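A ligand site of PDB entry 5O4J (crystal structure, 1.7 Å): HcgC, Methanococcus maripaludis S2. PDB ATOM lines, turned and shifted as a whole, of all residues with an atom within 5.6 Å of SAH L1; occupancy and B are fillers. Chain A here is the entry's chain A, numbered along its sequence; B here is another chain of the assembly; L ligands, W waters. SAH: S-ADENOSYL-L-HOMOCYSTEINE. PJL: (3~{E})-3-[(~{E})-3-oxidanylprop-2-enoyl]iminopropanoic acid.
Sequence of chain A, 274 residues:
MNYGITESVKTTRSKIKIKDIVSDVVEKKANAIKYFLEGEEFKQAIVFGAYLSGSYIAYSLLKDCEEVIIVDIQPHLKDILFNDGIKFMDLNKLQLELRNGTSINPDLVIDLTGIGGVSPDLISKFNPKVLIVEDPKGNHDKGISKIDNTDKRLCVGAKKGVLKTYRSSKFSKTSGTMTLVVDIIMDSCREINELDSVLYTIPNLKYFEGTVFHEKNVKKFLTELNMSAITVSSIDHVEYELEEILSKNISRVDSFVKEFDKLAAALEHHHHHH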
ATOM      1  N   LYS A  29      37.286 -39.326 -15.719  1.00  0.00           N
ATOM      2  CA  LYS A  29      36.056 -39.017 -14.998  1.00  0.00           C
ATOM      3  C   LYS A  29      35.007 -40.113 -15.209  1.00  0.00           C
ATOM      4  O   LYS A  29      34.343 -40.538 -14.251  1.00  0.00           O
ATOM      5  CB  LYS A  29      35.515 -37.653 -15.433  1.00  0.00           C
ATOM      6  CG  LYS A  29      36.421 -36.481 -15.074  1.00  0.00           C
ATOM      7  CD  LYS A  29      35.785 -35.146 -15.388  1.00  0.00           C
ATOM      8  CE  LYS A  29      36.690 -34.007 -14.915  1.00  0.00           C
ATOM      9  NZ  LYS A  29      36.045 -32.669 -15.079  1.00  0.00           N
ATOM     10  N   PHE A  48      23.144 -33.970 -16.099  1.00  0.00           N
ATOM     11  CA  PHE A  48      23.072 -32.527 -16.305  1.00  0.00           C
ATOM     12  C   PHE A  48      24.440 -31.995 -16.688  1.00  0.00           C
ATOM     13  O   PHE A  48      25.429 -32.218 -15.977  1.00  0.00           O
ATOM     14  CB  PHE A  48      22.574 -31.820 -15.039  1.00  0.00           C
ATOM     15  CG  PHE A  48      21.143 -32.103 -14.695  1.00  0.00           C
ATOM     16  CD1 PHE A  48      20.122 -31.354 -15.231  1.00  0.00           C
ATOM     17  CD2 PHE A  48      20.831 -33.125 -13.812  1.00  0.00           C
ATOM     18  CE1 PHE A  48      18.802 -31.610 -14.906  1.00  0.00           C
ATOM     19  CE2 PHE A  48      19.515 -33.390 -13.486  1.00  0.00           C
ATOM     20  CZ  PHE A  48      18.504 -32.637 -14.033  1.00  0.00           C
ATOM     21  N   GLY A  49      24.501 -31.290 -17.827  1.00  0.00           N
ATOM     22  CA  GLY A  49      25.730 -30.660 -18.275  1.00  0.00           C
ATOM     23  C   GLY A  49      26.421 -31.435 -19.387  1.00  0.00           C
ATOM     24  O   GLY A  49      27.148 -32.387 -19.121  1.00  0.00           O
ATOM     25  N   ALA A  50      26.171 -31.038 -20.625  1.00  0.00           N
ATOM     26  CA  ALA A  50      26.734 -31.752 -21.778  1.00  0.00           C
ATOM     27  C   ALA A  50      28.199 -31.421 -21.985  1.00  0.00           C
ATOM     28  O   ALA A  50      28.995 -32.284 -22.350  1.00  0.00           O
ATOM     29  CB  ALA A  50      25.933 -31.420 -23.038  1.00  0.00           C
ATOM     30  N   TYR A  51      28.579 -30.163 -21.764  1.00  0.00           N
ATOM     31  CA  TYR A  51      29.946 -29.721 -21.936  1.00  0.00           C
ATOM     32  C   TYR A  51      30.687 -29.823 -20.602  1.00  0.00           C
ATOM     33  O   TYR A  51      30.072 -29.525 -19.568  1.00  0.00           O
ATOM     34  CB  TYR A  51      29.951 -28.286 -22.460  1.00  0.00           C
ATOM     35  CG  TYR A  51      31.287 -27.577 -22.400  1.00  0.00           C
ATOM     36  CD1 TYR A  51      31.697 -26.950 -21.235  1.00  0.00           C
ATOM     37  CD2 TYR A  51      32.100 -27.479 -23.510  1.00  0.00           C
ATOM     38  CE1 TYR A  51      32.888 -26.289 -21.165  1.00  0.00           C
ATOM     39  CE2 TYR A  51      33.296 -26.807 -23.461  1.00  0.00           C
ATOM     40  CZ  TYR A  51      33.694 -26.219 -22.282  1.00  0.00           C
ATOM     41  OH  TYR A  51      34.907 -25.537 -22.233  1.00  0.00           O
ATOM     42  N   LEU A  52      31.948 -30.250 -20.555  1.00  0.00           N
ATOM     43  CA  LEU A  52      32.733 -30.787 -21.679  1.00  0.00           C
ATOM     44  C   LEU A  52      32.830 -32.318 -21.563  1.00  0.00           C
ATOM     45  O   LEU A  52      32.890 -33.013 -22.564  1.00  0.00           O
ATOM     46  CB  LEU A  52      34.125 -30.158 -21.679  1.00  0.00           C
ATOM     47  CG  LEU A  52      35.139 -30.609 -22.723  1.00  0.00           C
ATOM     48  CD1 LEU A  52      34.551 -30.615 -24.131  1.00  0.00           C
ATOM     49  CD2 LEU A  52      36.384 -29.721 -22.665  1.00  0.00           C
ATOM     50  N   SER A  53      32.855 -32.846 -20.329  1.00  0.00           N
ATOM     51  CA  SER A  53      32.941 -34.293 -20.132  1.00  0.00           C
ATOM     52  C   SER A  53      31.585 -34.987 -20.165  1.00  0.00           C
ATOM     53  O   SER A  53      31.541 -36.220 -20.257  1.00  0.00           O
ATOM     54  CB  SER A  53      33.628 -34.624 -18.806  1.00  0.00           C
ATOM     55  OG  SER A  53      33.969 -33.474 -18.062  1.00  0.00           O
ATOM     56  N   GLY A  54      30.484 -34.228 -20.071  1.00  0.00           N
ATOM     57  CA  GLY A  54      29.170 -34.848 -19.989  1.00  0.00           C
ATOM     58  C   GLY A  54      28.853 -35.759 -21.161  1.00  0.00           C
ATOM     59  O   GLY A  54      28.271 -36.828 -20.986  1.00  0.00           O
ATOM     60  N   VAL A  71      20.784 -33.486 -20.174  1.00  0.00           N
ATOM     61  CA  VAL A  71      20.020 -32.249 -20.040  1.00  0.00           C
ATOM     62  C   VAL A  71      21.013 -31.103 -20.007  1.00  0.00           C
ATOM     63  O   VAL A  71      21.981 -31.147 -19.255  1.00  0.00           O
ATOM     64  CB  VAL A  71      19.133 -32.231 -18.783  1.00  0.00           C
ATOM     65  CG1 VAL A  71      18.413 -30.889 -18.658  1.00  0.00           C
ATOM     66  CG2 VAL A  71      18.146 -33.386 -18.815  1.00  0.00           C
ATOM     67  N   ASP A  72      20.769 -30.094 -20.837  1.00  0.00           N
ATOM     68  CA  ASP A  72      21.565 -28.886 -20.797  1.00  0.00           C
ATOM     69  C   ASP A  72      20.682 -27.676 -20.976  1.00  0.00           C
ATOM     70  O   ASP A  72      19.718 -27.702 -21.750  1.00  0.00           O
ATOM     71  CB  ASP A  72      22.665 -28.884 -21.857  1.00  0.00           C
ATOM     72  CG  ASP A  72      23.824 -27.991 -21.460  1.00  0.00           C
ATOM     73  OD1 ASP A  72      23.684 -26.746 -21.537  1.00  0.00           O
ATOM     74  OD2 ASP A  72      24.862 -28.532 -21.016  1.00  0.00           O
ATOM     75  N   ILE A  73      21.001 -26.611 -20.253  1.00  0.00           N
ATOM     76  CA  ILE A  73      20.280 -25.358 -20.370  1.00  0.00           C
ATOM     77  C   ILE A  73      20.472 -24.734 -21.738  1.00  0.00           C
ATOM     78  O   ILE A  73      19.634 -23.936 -22.172  1.00  0.00           O
ATOM     79  CB  ILE A  73      20.720 -24.403 -19.229  1.00  0.00           C
ATOM     80  CG1 ILE A  73      19.723 -23.243 -19.094  1.00  0.00           C
ATOM     81  CG2 ILE A  73      22.133 -23.883 -19.448  1.00  0.00           C
ATOM     82  CD1 ILE A  73      19.885 -22.497 -17.779  1.00  0.00           C
ATOM     83  N   GLN A  74      21.540 -25.102 -22.457  1.00  0.00           N
ATOM     84  CA  GLN A  74      21.823 -24.572 -23.792  1.00  0.00           C
ATOM     85  C   GLN A  74      21.301 -25.561 -24.832  1.00  0.00           C
ATOM     86  O   GLN A  74      21.881 -26.640 -24.989  1.00  0.00           O
ATOM     87  CB  GLN A  74      23.326 -24.367 -23.975  1.00  0.00           C
ATOM     88  CG  GLN A  74      23.958 -23.392 -23.000  1.00  0.00           C
ATOM     89  CD  GLN A  74      23.739 -21.943 -23.403  1.00  0.00           C
ATOM     90  OE1 GLN A  74      23.662 -21.626 -24.596  1.00  0.00           O
ATOM     91  NE2 GLN A  74      23.654 -21.066 -22.412  1.00  0.00           N
ATOM     92  N   LEU A  77      23.705 -27.305 -27.474  1.00  0.00           N
ATOM     93  CA  LEU A  77      24.667 -28.342 -27.110  1.00  0.00           C
ATOM     94  C   LEU A  77      24.201 -29.737 -27.480  1.00  0.00           C
ATOM     95  O   LEU A  77      24.951 -30.694 -27.263  1.00  0.00           O
ATOM     96  CB  LEU A  77      24.994 -28.257 -25.629  1.00  0.00           C
ATOM     97  CG  LEU A  77      26.055 -27.198 -25.303  1.00  0.00           C
ATOM     98  CD1 LEU A  77      26.198 -27.055 -23.804  1.00  0.00           C
ATOM     99  CD2 LEU A  77      27.402 -27.545 -25.935  1.00  0.00           C
ATOM    100  N   LEU A  91      16.756 -27.734 -20.689  1.00  0.00           N
ATOM    101  CA  LEU A  91      16.250 -27.611 -19.331  1.00  0.00           C
ATOM    102  C   LEU A  91      14.753 -27.314 -19.332  1.00  0.00           C
ATOM    103  O   LEU A  91      14.001 -27.854 -18.515  1.00  0.00           O
ATOM    104  CB  LEU A  91      17.025 -26.536 -18.583  1.00  0.00           C
ATOM    105  CG  LEU A  91      16.738 -26.386 -17.090  1.00  0.00           C
ATOM    106  CD1 LEU A  91      16.998 -27.689 -16.359  1.00  0.00           C
ATOM    107  CD2 LEU A  91      17.578 -25.269 -16.496  1.00  0.00           C
ATOM    108  N   LEU A 112      26.798 -32.619 -13.534  1.00  0.00           N
ATOM    109  CA  LEU A 112      28.126 -32.220 -13.964  1.00  0.00           C
ATOM    110  C   LEU A 112      28.232 -30.727 -14.210  1.00  0.00           C
ATOM    111  O   LEU A 112      29.225 -30.275 -14.798  1.00  0.00           O
ATOM    112  CB  LEU A 112      28.494 -32.983 -15.249  1.00  0.00           C
ATOM    113  CG  LEU A 112      28.421 -34.500 -15.161  1.00  0.00           C
ATOM    114  CD1 LEU A 112      28.658 -35.138 -16.524  1.00  0.00           C
ATOM    115  CD2 LEU A 112      29.438 -35.019 -14.166  1.00  0.00           C
ATOM    116  N   THR A 113      27.249 -29.937 -13.763  1.00  0.00           N
ATOM    117  CA  THR A 113      27.199 -28.543 -14.174  1.00  0.00           C
ATOM    118  C   THR A 113      28.170 -27.666 -13.410  1.00  0.00           C
ATOM    119  O   THR A 113      28.596 -26.625 -13.918  1.00  0.00           O
ATOM    120  CB  THR A 113      25.781 -27.975 -14.051  1.00  0.00           C
ATOM    121  OG1 THR A 113      25.331 -28.030 -12.692  1.00  0.00           O
ATOM    122  CG2 THR A 113      24.821 -28.756 -14.936  1.00  0.00           C
ATOM    123  N   GLY A 114      28.522 -28.040 -12.181  1.00  0.00           N
ATOM    124  CA  GLY A 114      29.519 -27.291 -11.442  1.00  0.00           C
ATOM    125  C   GLY A 114      29.067 -25.867 -11.156  1.00  0.00           C
ATOM    126  O   GLY A 114      27.914 -25.610 -10.839  1.00  0.00           O
ATOM    127  N   GLY A 116      27.701 -22.339 -10.731  1.00  0.00           N
ATOM    128  CA  GLY A 116      26.545 -21.657 -11.265  1.00  0.00           C
ATOM    129  C   GLY A 116      25.570 -22.544 -11.998  1.00  0.00           C
ATOM    130  O   GLY A 116      24.731 -22.041 -12.744  1.00  0.00           O
ATOM    131  N   GLY A 117      25.624 -23.853 -11.757  1.00  0.00           N
ATOM    132  CA  GLY A 117      24.818 -24.816 -12.487  1.00  0.00           C
ATOM    133  C   GLY A 117      23.453 -25.120 -11.877  1.00  0.00           C
ATOM    134  O   GLY A 117      22.745 -24.207 -11.434  1.00  0.00           O
ATOM    135  N   VAL A 118      23.063 -26.391 -11.886  1.00  0.00           N
ATOM    136  CA  VAL A 118      21.721 -26.766 -11.478  1.00  0.00           C
ATOM    137  C   VAL A 118      21.484 -26.383 -10.018  1.00  0.00           C
ATOM    138  O   VAL A 118      22.398 -26.389  -9.181  1.00  0.00           O
ATOM    139  CB  VAL A 118      21.449 -28.270 -11.660  1.00  0.00           C
ATOM    140  CG1 VAL A 118      21.588 -28.663 -13.113  1.00  0.00           C
ATOM    141  CG2 VAL A 118      22.357 -29.087 -10.778  1.00  0.00           C
ATOM    142  N   SER A 119      20.257 -26.101  -9.717  1.00  0.00           N
ATOM    143  CA  SER A 119      19.865 -25.694  -8.375  1.00  0.00           C
ATOM    144  C   SER A 119      19.565 -26.921  -7.520  1.00  0.00           C
ATOM    145  O   SER A 119      19.071 -27.932  -8.023  1.00  0.00           O
ATOM    146  CB  SER A 119      18.621 -24.816  -8.429  1.00  0.00           C
ATOM    147  OG  SER A 119      17.500 -25.575  -8.859  1.00  0.00           O
ATOM    148  N   LEU A 122      16.009 -28.088  -8.150  1.00  0.00           N
ATOM    149  CA  LEU A 122      15.717 -28.999  -9.250  1.00  0.00           C
ATOM    150  C   LEU A 122      16.144 -30.432  -8.933  1.00  0.00           C
ATOM    151  O   LEU A 122      15.416 -31.388  -9.228  1.00  0.00           O
ATOM    152  CB  LEU A 122      16.395 -28.512 -10.527  1.00  0.00           C
ATOM    153  CG  LEU A 122      16.259 -29.419 -11.753  1.00  0.00           C
ATOM    154  CD1 LEU A 122      14.798 -29.624 -12.133  1.00  0.00           C
ATOM    155  CD2 LEU A 122      17.031 -28.831 -12.936  1.00  0.00           C
ATOM    156  N   GLU A 134      29.285 -33.564  -9.456  1.00  0.00           N
ATOM    157  CA  GLU A 134      30.679 -33.230  -9.686  1.00  0.00           C
ATOM    158  C   GLU A 134      31.044 -31.999  -8.869  1.00  0.00           C
ATOM    159  O   GLU A 134      30.362 -30.973  -8.940  1.00  0.00           O
ATOM    160  CB  GLU A 134      30.970 -33.004 -11.169  1.00  0.00           C
ATOM    161  CG  GLU A 134      32.453 -32.747 -11.408  1.00  0.00           C
ATOM    162  CD  GLU A 134      32.833 -32.735 -12.866  1.00  0.00           C
ATOM    163  OE1 GLU A 134      31.934 -32.595 -13.726  1.00  0.00           O
ATOM    164  OE2 GLU A 134      34.044 -32.849 -13.145  1.00  0.00           O
ATOM    165  N   SER A 175      38.291 -28.514 -11.087  1.00  0.00           N
ATOM    166  CA  SER A 175      38.283 -29.854 -11.640  1.00  0.00           C
ATOM    167  C   SER A 175      37.710 -29.907 -13.042  1.00  0.00           C
ATOM    168  O   SER A 175      37.517 -31.003 -13.576  1.00  0.00           O
ATOM    169  CB  SER A 175      37.443 -30.759 -10.737  1.00  0.00           C
ATOM    170  OG  SER A 175      36.144 -30.200 -10.669  1.00  0.00           O
ATOM    171  N   GLY A 176      37.356 -28.753 -13.599  1.00  0.00           N
ATOM    172  CA  GLY A 176      36.746 -28.737 -14.919  1.00  0.00           C
ATOM    173  C   GLY A 176      37.704 -29.291 -15.965  1.00  0.00           C
ATOM    174  O   GLY A 176      38.917 -29.071 -15.907  1.00  0.00           O
ATOM    175  N   THR A 177      37.146 -30.013 -16.934  1.00  0.00           N
ATOM    176  CA  THR A 177      37.967 -30.591 -18.002  1.00  0.00           C
ATOM    177  C   THR A 177      38.804 -29.508 -18.682  1.00  0.00           C
ATOM    178  O   THR A 177      40.008 -29.686 -18.874  1.00  0.00           O
ATOM    179  CB  THR A 177      37.079 -31.321 -18.991  1.00  0.00           C
ATOM    180  OG1 THR A 177      36.308 -32.315 -18.277  1.00  0.00           O
ATOM    181  CG2 THR A 177      37.890 -32.022 -20.076  1.00  0.00           C
ATOM    182  N   MET A 178      38.182 -28.381 -19.054  1.00  0.00           N
ATOM    183  CA  MET A 178      38.906 -27.302 -19.708  1.00  0.00           C
ATOM    184  C   MET A 178      40.052 -26.787 -18.838  1.00  0.00           C
ATOM    185  O   MET A 178      41.171 -26.609 -19.323  1.00  0.00           O
ATOM    186  CB  MET A 178      37.950 -26.154 -20.043  1.00  0.00           C
ATOM    187  CG  MET A 178      38.606 -24.959 -20.751  1.00  0.00           C
ATOM    188  SD  MET A 178      39.477 -25.343 -22.271  1.00  0.00           S
ATOM    189  CE  MET A 178      38.189 -26.159 -23.214  1.00  0.00           C
ATOM    190  N   PHE A 213      30.044 -21.348 -26.182  1.00  0.00           N
ATOM    191  CA  PHE A 213      28.963 -20.694 -25.442  1.00  0.00           C
ATOM    192  C   PHE A 213      28.649 -19.284 -25.905  1.00  0.00           C
ATOM    193  O   PHE A 213      27.550 -18.803 -25.620  1.00  0.00           O
ATOM    194  CB  PHE A 213      29.297 -20.663 -23.955  1.00  0.00           C
ATOM    195  CG  PHE A 213      29.272 -22.018 -23.350  1.00  0.00           C
ATOM    196  CD1 PHE A 213      28.081 -22.577 -22.968  1.00  0.00           C
ATOM    197  CD2 PHE A 213      30.445 -22.772 -23.270  1.00  0.00           C
ATOM    198  CE1 PHE A 213      28.031 -23.854 -22.462  1.00  0.00           C
ATOM    199  CE2 PHE A 213      30.400 -24.057 -22.753  1.00  0.00           C
ATOM    200  CZ  PHE A 213      29.198 -24.597 -22.364  1.00  0.00           C
ATOM    201  N   ILE B   5      30.253 -19.421 -19.004  1.00  0.00           N
ATOM    202  CA  ILE B   5      29.265 -20.446 -19.301  1.00  0.00           C
ATOM    203  C   ILE B   5      27.914 -20.113 -18.677  1.00  0.00           C
ATOM    204  O   ILE B   5      26.855 -20.423 -19.233  1.00  0.00           O
ATOM    205  CB  ILE B   5      29.786 -21.816 -18.826  1.00  0.00           C
ATOM    206  CG1 ILE B   5      31.038 -22.206 -19.638  1.00  0.00           C
ATOM    207  CG2 ILE B   5      28.696 -22.873 -18.901  1.00  0.00           C
ATOM    208  CD1 ILE B   5      31.780 -23.414 -19.072  1.00  0.00           C
ATOM    209  N   THR B   6      27.934 -19.489 -17.495  1.00  0.00           N
ATOM    210  CA  THR B   6      26.765 -18.966 -16.835  1.00  0.00           C
ATOM    211  C   THR B   6      27.093 -17.565 -16.339  1.00  0.00           C
ATOM    212  O   THR B   6      28.215 -17.095 -16.462  1.00  0.00           O
ATOM    213  CB  THR B   6      26.330 -19.820 -15.632  1.00  0.00           C
ATOM    214  OG1 THR B   6      27.285 -19.625 -14.575  1.00  0.00           O
ATOM    215  CG2 THR B   6      26.246 -21.299 -16.012  1.00  0.00           C
HETATM  216  N   SAH L   1      32.395 -29.796 -14.923  1.00  0.00           N
HETATM  217  CA  SAH L   1      32.313 -29.845 -16.410  1.00  0.00           C
HETATM  218  CB  SAH L   1      32.060 -28.445 -16.959  1.00  0.00           C
HETATM  219  CG  SAH L   1      30.605 -28.031 -16.780  1.00  0.00           C
HETATM  220  SD  SAH L   1      30.272 -26.461 -17.542  1.00  0.00           S
HETATM  221  C   SAH L   1      33.572 -30.380 -17.025  1.00  0.00           C
HETATM  222  O   SAH L   1      33.651 -30.456 -18.272  1.00  0.00           O
HETATM  223  OXT SAH L   1      34.490 -30.719 -16.264  1.00  0.00           O
HETATM  224  C5' SAH L   1      28.525 -26.297 -17.266  1.00  0.00           C
HETATM  225  C4' SAH L   1      27.686 -27.113 -18.254  1.00  0.00           C
HETATM  226  O4' SAH L   1      26.387 -27.314 -17.673  1.00  0.00           O
HETATM  227  C3' SAH L   1      27.447 -26.356 -19.540  1.00  0.00           C
HETATM  228  O3' SAH L   1      27.249 -27.248 -20.649  1.00  0.00           O
HETATM  229  C2' SAH L   1      26.199 -25.572 -19.212  1.00  0.00           C
HETATM  230  O2' SAH L   1      25.468 -25.115 -20.352  1.00  0.00           O
HETATM  231  C1' SAH L   1      25.410 -26.590 -18.426  1.00  0.00           C
HETATM  232  N9  SAH L   1      24.473 -25.997 -17.444  1.00  0.00           N
HETATM  233  C8  SAH L   1      24.706 -24.918 -16.666  1.00  0.00           C
HETATM  234  N7  SAH L   1      23.622 -24.700 -15.870  1.00  0.00           N
HETATM  235  C5  SAH L   1      22.728 -25.667 -16.139  1.00  0.00           C
HETATM  236  C6  SAH L   1      21.383 -26.033 -15.643  1.00  0.00           C
HETATM  237  N6  SAH L   1      20.780 -25.297 -14.685  1.00  0.00           N
HETATM  238  N1  SAH L   1      20.791 -27.117 -16.192  1.00  0.00           N
HETATM  239  C2  SAH L   1      21.382 -27.870 -17.138  1.00  0.00           C
HETATM  240  N3  SAH L   1      22.602 -27.588 -17.630  1.00  0.00           N
HETATM  241  C4  SAH L   1      23.297 -26.526 -17.176  1.00  0.00           C
HETATM  242  O14 PJL L   2      35.078 -25.547 -17.457  1.00  0.00           O
HETATM  243  C12 PJL L   2      35.983 -25.257 -16.622  1.00  0.00           C
HETATM  244  O13 PJL L   2      37.057 -25.877 -16.510  1.00  0.00           O
HETATM  245  C10 PJL L   2      35.847 -24.110 -15.652  1.00  0.00           C
HETATM  246  C4  PJL L   2      34.437 -23.919 -15.146  1.00  0.00           C
HETATM  247  N5  PJL L   2      33.586 -23.250 -15.799  1.00  0.00           N
HETATM  248  C6  PJL L   2      32.325 -23.042 -15.381  1.00  0.00           C
HETATM  249  O8  PJL L   2      31.714 -22.032 -15.720  1.00  0.00           O
HETATM  250  C7  PJL L   2      31.632 -24.003 -14.487  1.00  0.00           C
HETATM  251  C2  PJL L   2      32.237 -25.097 -14.049  1.00  0.00           C
HETATM  252  O1  PJL L   2      31.662 -25.967 -13.241  1.00  0.00           O
HETATM  253  O   HOH W   1      35.386 -27.978 -18.809  1.00  0.00           O
HETATM  254  O   HOH W   2      25.033 -22.350 -20.016  1.00  0.00           O
HETATM  255  O   HOH W   3      31.756 -33.098 -16.455  1.00  0.00           O
HETATM  256  O   HOH W   4      18.704 -25.344 -12.274  1.00  0.00           O
HETATM  257  O   HOH W   5      22.688 -22.383 -14.497  1.00  0.00           O
HETATM  258  O   HOH W   6      27.292 -24.352 -14.797  1.00  0.00           O
HETATM  259  O   HOH W   7      34.380 -29.995 -12.682  1.00  0.00           O
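The backbone NH (N) of Gln 74 sits at hydrogen-bond distance from the side-chain carboxylate (OD1) of Asp 72 (2.9 Å). The backbone carbonyl oxygen of Asp 72 lies within hydrogen-bond range of the backbone NH of Leu 91 (3.1 Å). OD2 of Asp 72 sits at hydrogen-bond distance from N of Ala 50 (2.9 Å). NZ of Lys 29 is in salt-bridge range of OE2 of Glu 134, at 2.8 Å. NZ of Lys 29 sits at hydrogen-bond distance from O of Ser 175 (2.7 Å). The side-chain hydroxyl of Thr 177 lies within hydrogen-bond range of the side-chain hydroxyl of Ser 53, at 2.6 Å. The backbone NH (N) of Leu 112 lies within hydrogen-bond range of the backbone carbonyl oxygen (O) of Phe 48 (2.8 Å). OG1 of Thr 113 sits at hydrogen-bond distance from N of Val 118 (2.9 Å).
Water W2 lies within hydrogen-bond range of the backbone carbonyl oxygen of Ile 5 of chain B (2.8 Å), an oxygen (O2') of SAH L1 (2.8 Å) and the side-chain amide nitrogen of Gln 74 (3.0 Å). Water W5 lies within hydrogen-bond range of O of Gly 116 (2.7 Å) and N7 of SAH L1 (2.9 Å). Water W7 lies within hydrogen-bond range of OG of Ser 175 (2.7 Å), OE2 of Glu 134 (2.9 Å), N of SAH L1 (3.0 Å) and N of Gly 176 (3.4 Å). Water W1 lies within hydrogen-bond range of an oxygen (O14) of PJL L2 (2.8 Å), the backbone NH (N) of Met 178 (2.8 Å), an oxygen (O) of SAH L1 (3.1 Å) and the backbone NH (N) of Thr 177 (3.3 Å). Water W4 bridges the backbone NH of Ser 119 (3.1 Å) and a nitrogen (N6) of SAH L1 (3.2 Å). Water W3 lies within hydrogen-bond range of OG of Ser 53 and OE1 of Glu 134.
Residues that only touch SAH L1: Gly 176 (3.3 Å), Leu 77 (3.3 Å), Thr 113 (3.4 Å), Gly 49 (3.5 Å), Gln 74 (3.5 Å), Val 118 (3.5 Å), Phe 213 (3.6 Å), Gly 117 (3.6 Å), Leu 91 (3.7 Å), Ile 5 of chain B (3.7 Å), Ala 50 (3.9 Å), Val 71 (3.9 Å) and Thr 6 of chain B (3.99 Å). Hydrophobic or aromatic side chains that line SAH L1: Tyr 51, Leu 52, Ile 73, Leu 77, Leu 91, Val 118, Phe 213 and Ile 5 of chain B. Within 4 Å of SAH L1: Lys 29, Gly 49, Ala 50, Tyr 51, Leu 52, Ser 53, Val 71, Asp 72, Ile 73, Gln 74, Leu 77, Leu 91, Leu 112, Thr 113, Gly 117, Val 118, Glu 134, Gly 176, Thr 177, Phe 213, Ile 5 of chain B and Thr 6 of chain B.
O2' of SAH L1 lies within hydrogen-bond range of OD1 of Asp 72, at 2.7 Å. NZ of Lys 29 is in salt-bridge range of OXT of SAH L1, 2.8 Å away. An oxygen (OXT) of SAH L1 lies within hydrogen-bond range of the backbone NH (N) of Thr 177. The side-chain hydroxyl (OG1) of Thr 177 sits at hydrogen-bond distance from an oxygen (OXT) of SAH L1. An oxygen (O) of SAH L1 lies within hydrogen-bond range of the backbone NH (N) of Leu 52 (2.9 Å). N of Ser 53 sits at hydrogen-bond distance from O of SAH L1. OG of Ser 53 lies within hydrogen-bond range of O of SAH L1 (3.0 Å). The side-chain carboxylate (OE1) of Glu 134 lies within salt-bridge range of a nitrogen (N) of SAH L1 (3.1 Å). The backbone NH (N) of Tyr 51 sits at hydrogen-bond distance from an oxygen (O3') of SAH L1. The backbone carbonyl oxygen (O) of Leu 112 sits at hydrogen-bond distance from a nitrogen (N) of SAH L1 (3.2 Å). The backbone NH (N) of Ile 73 lies within hydrogen-bond range of a nitrogen (N3) of SAH L1 (3.2 Å). O1 of PJL L2 sits at hydrogen-bond distance from O of Thr 113.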
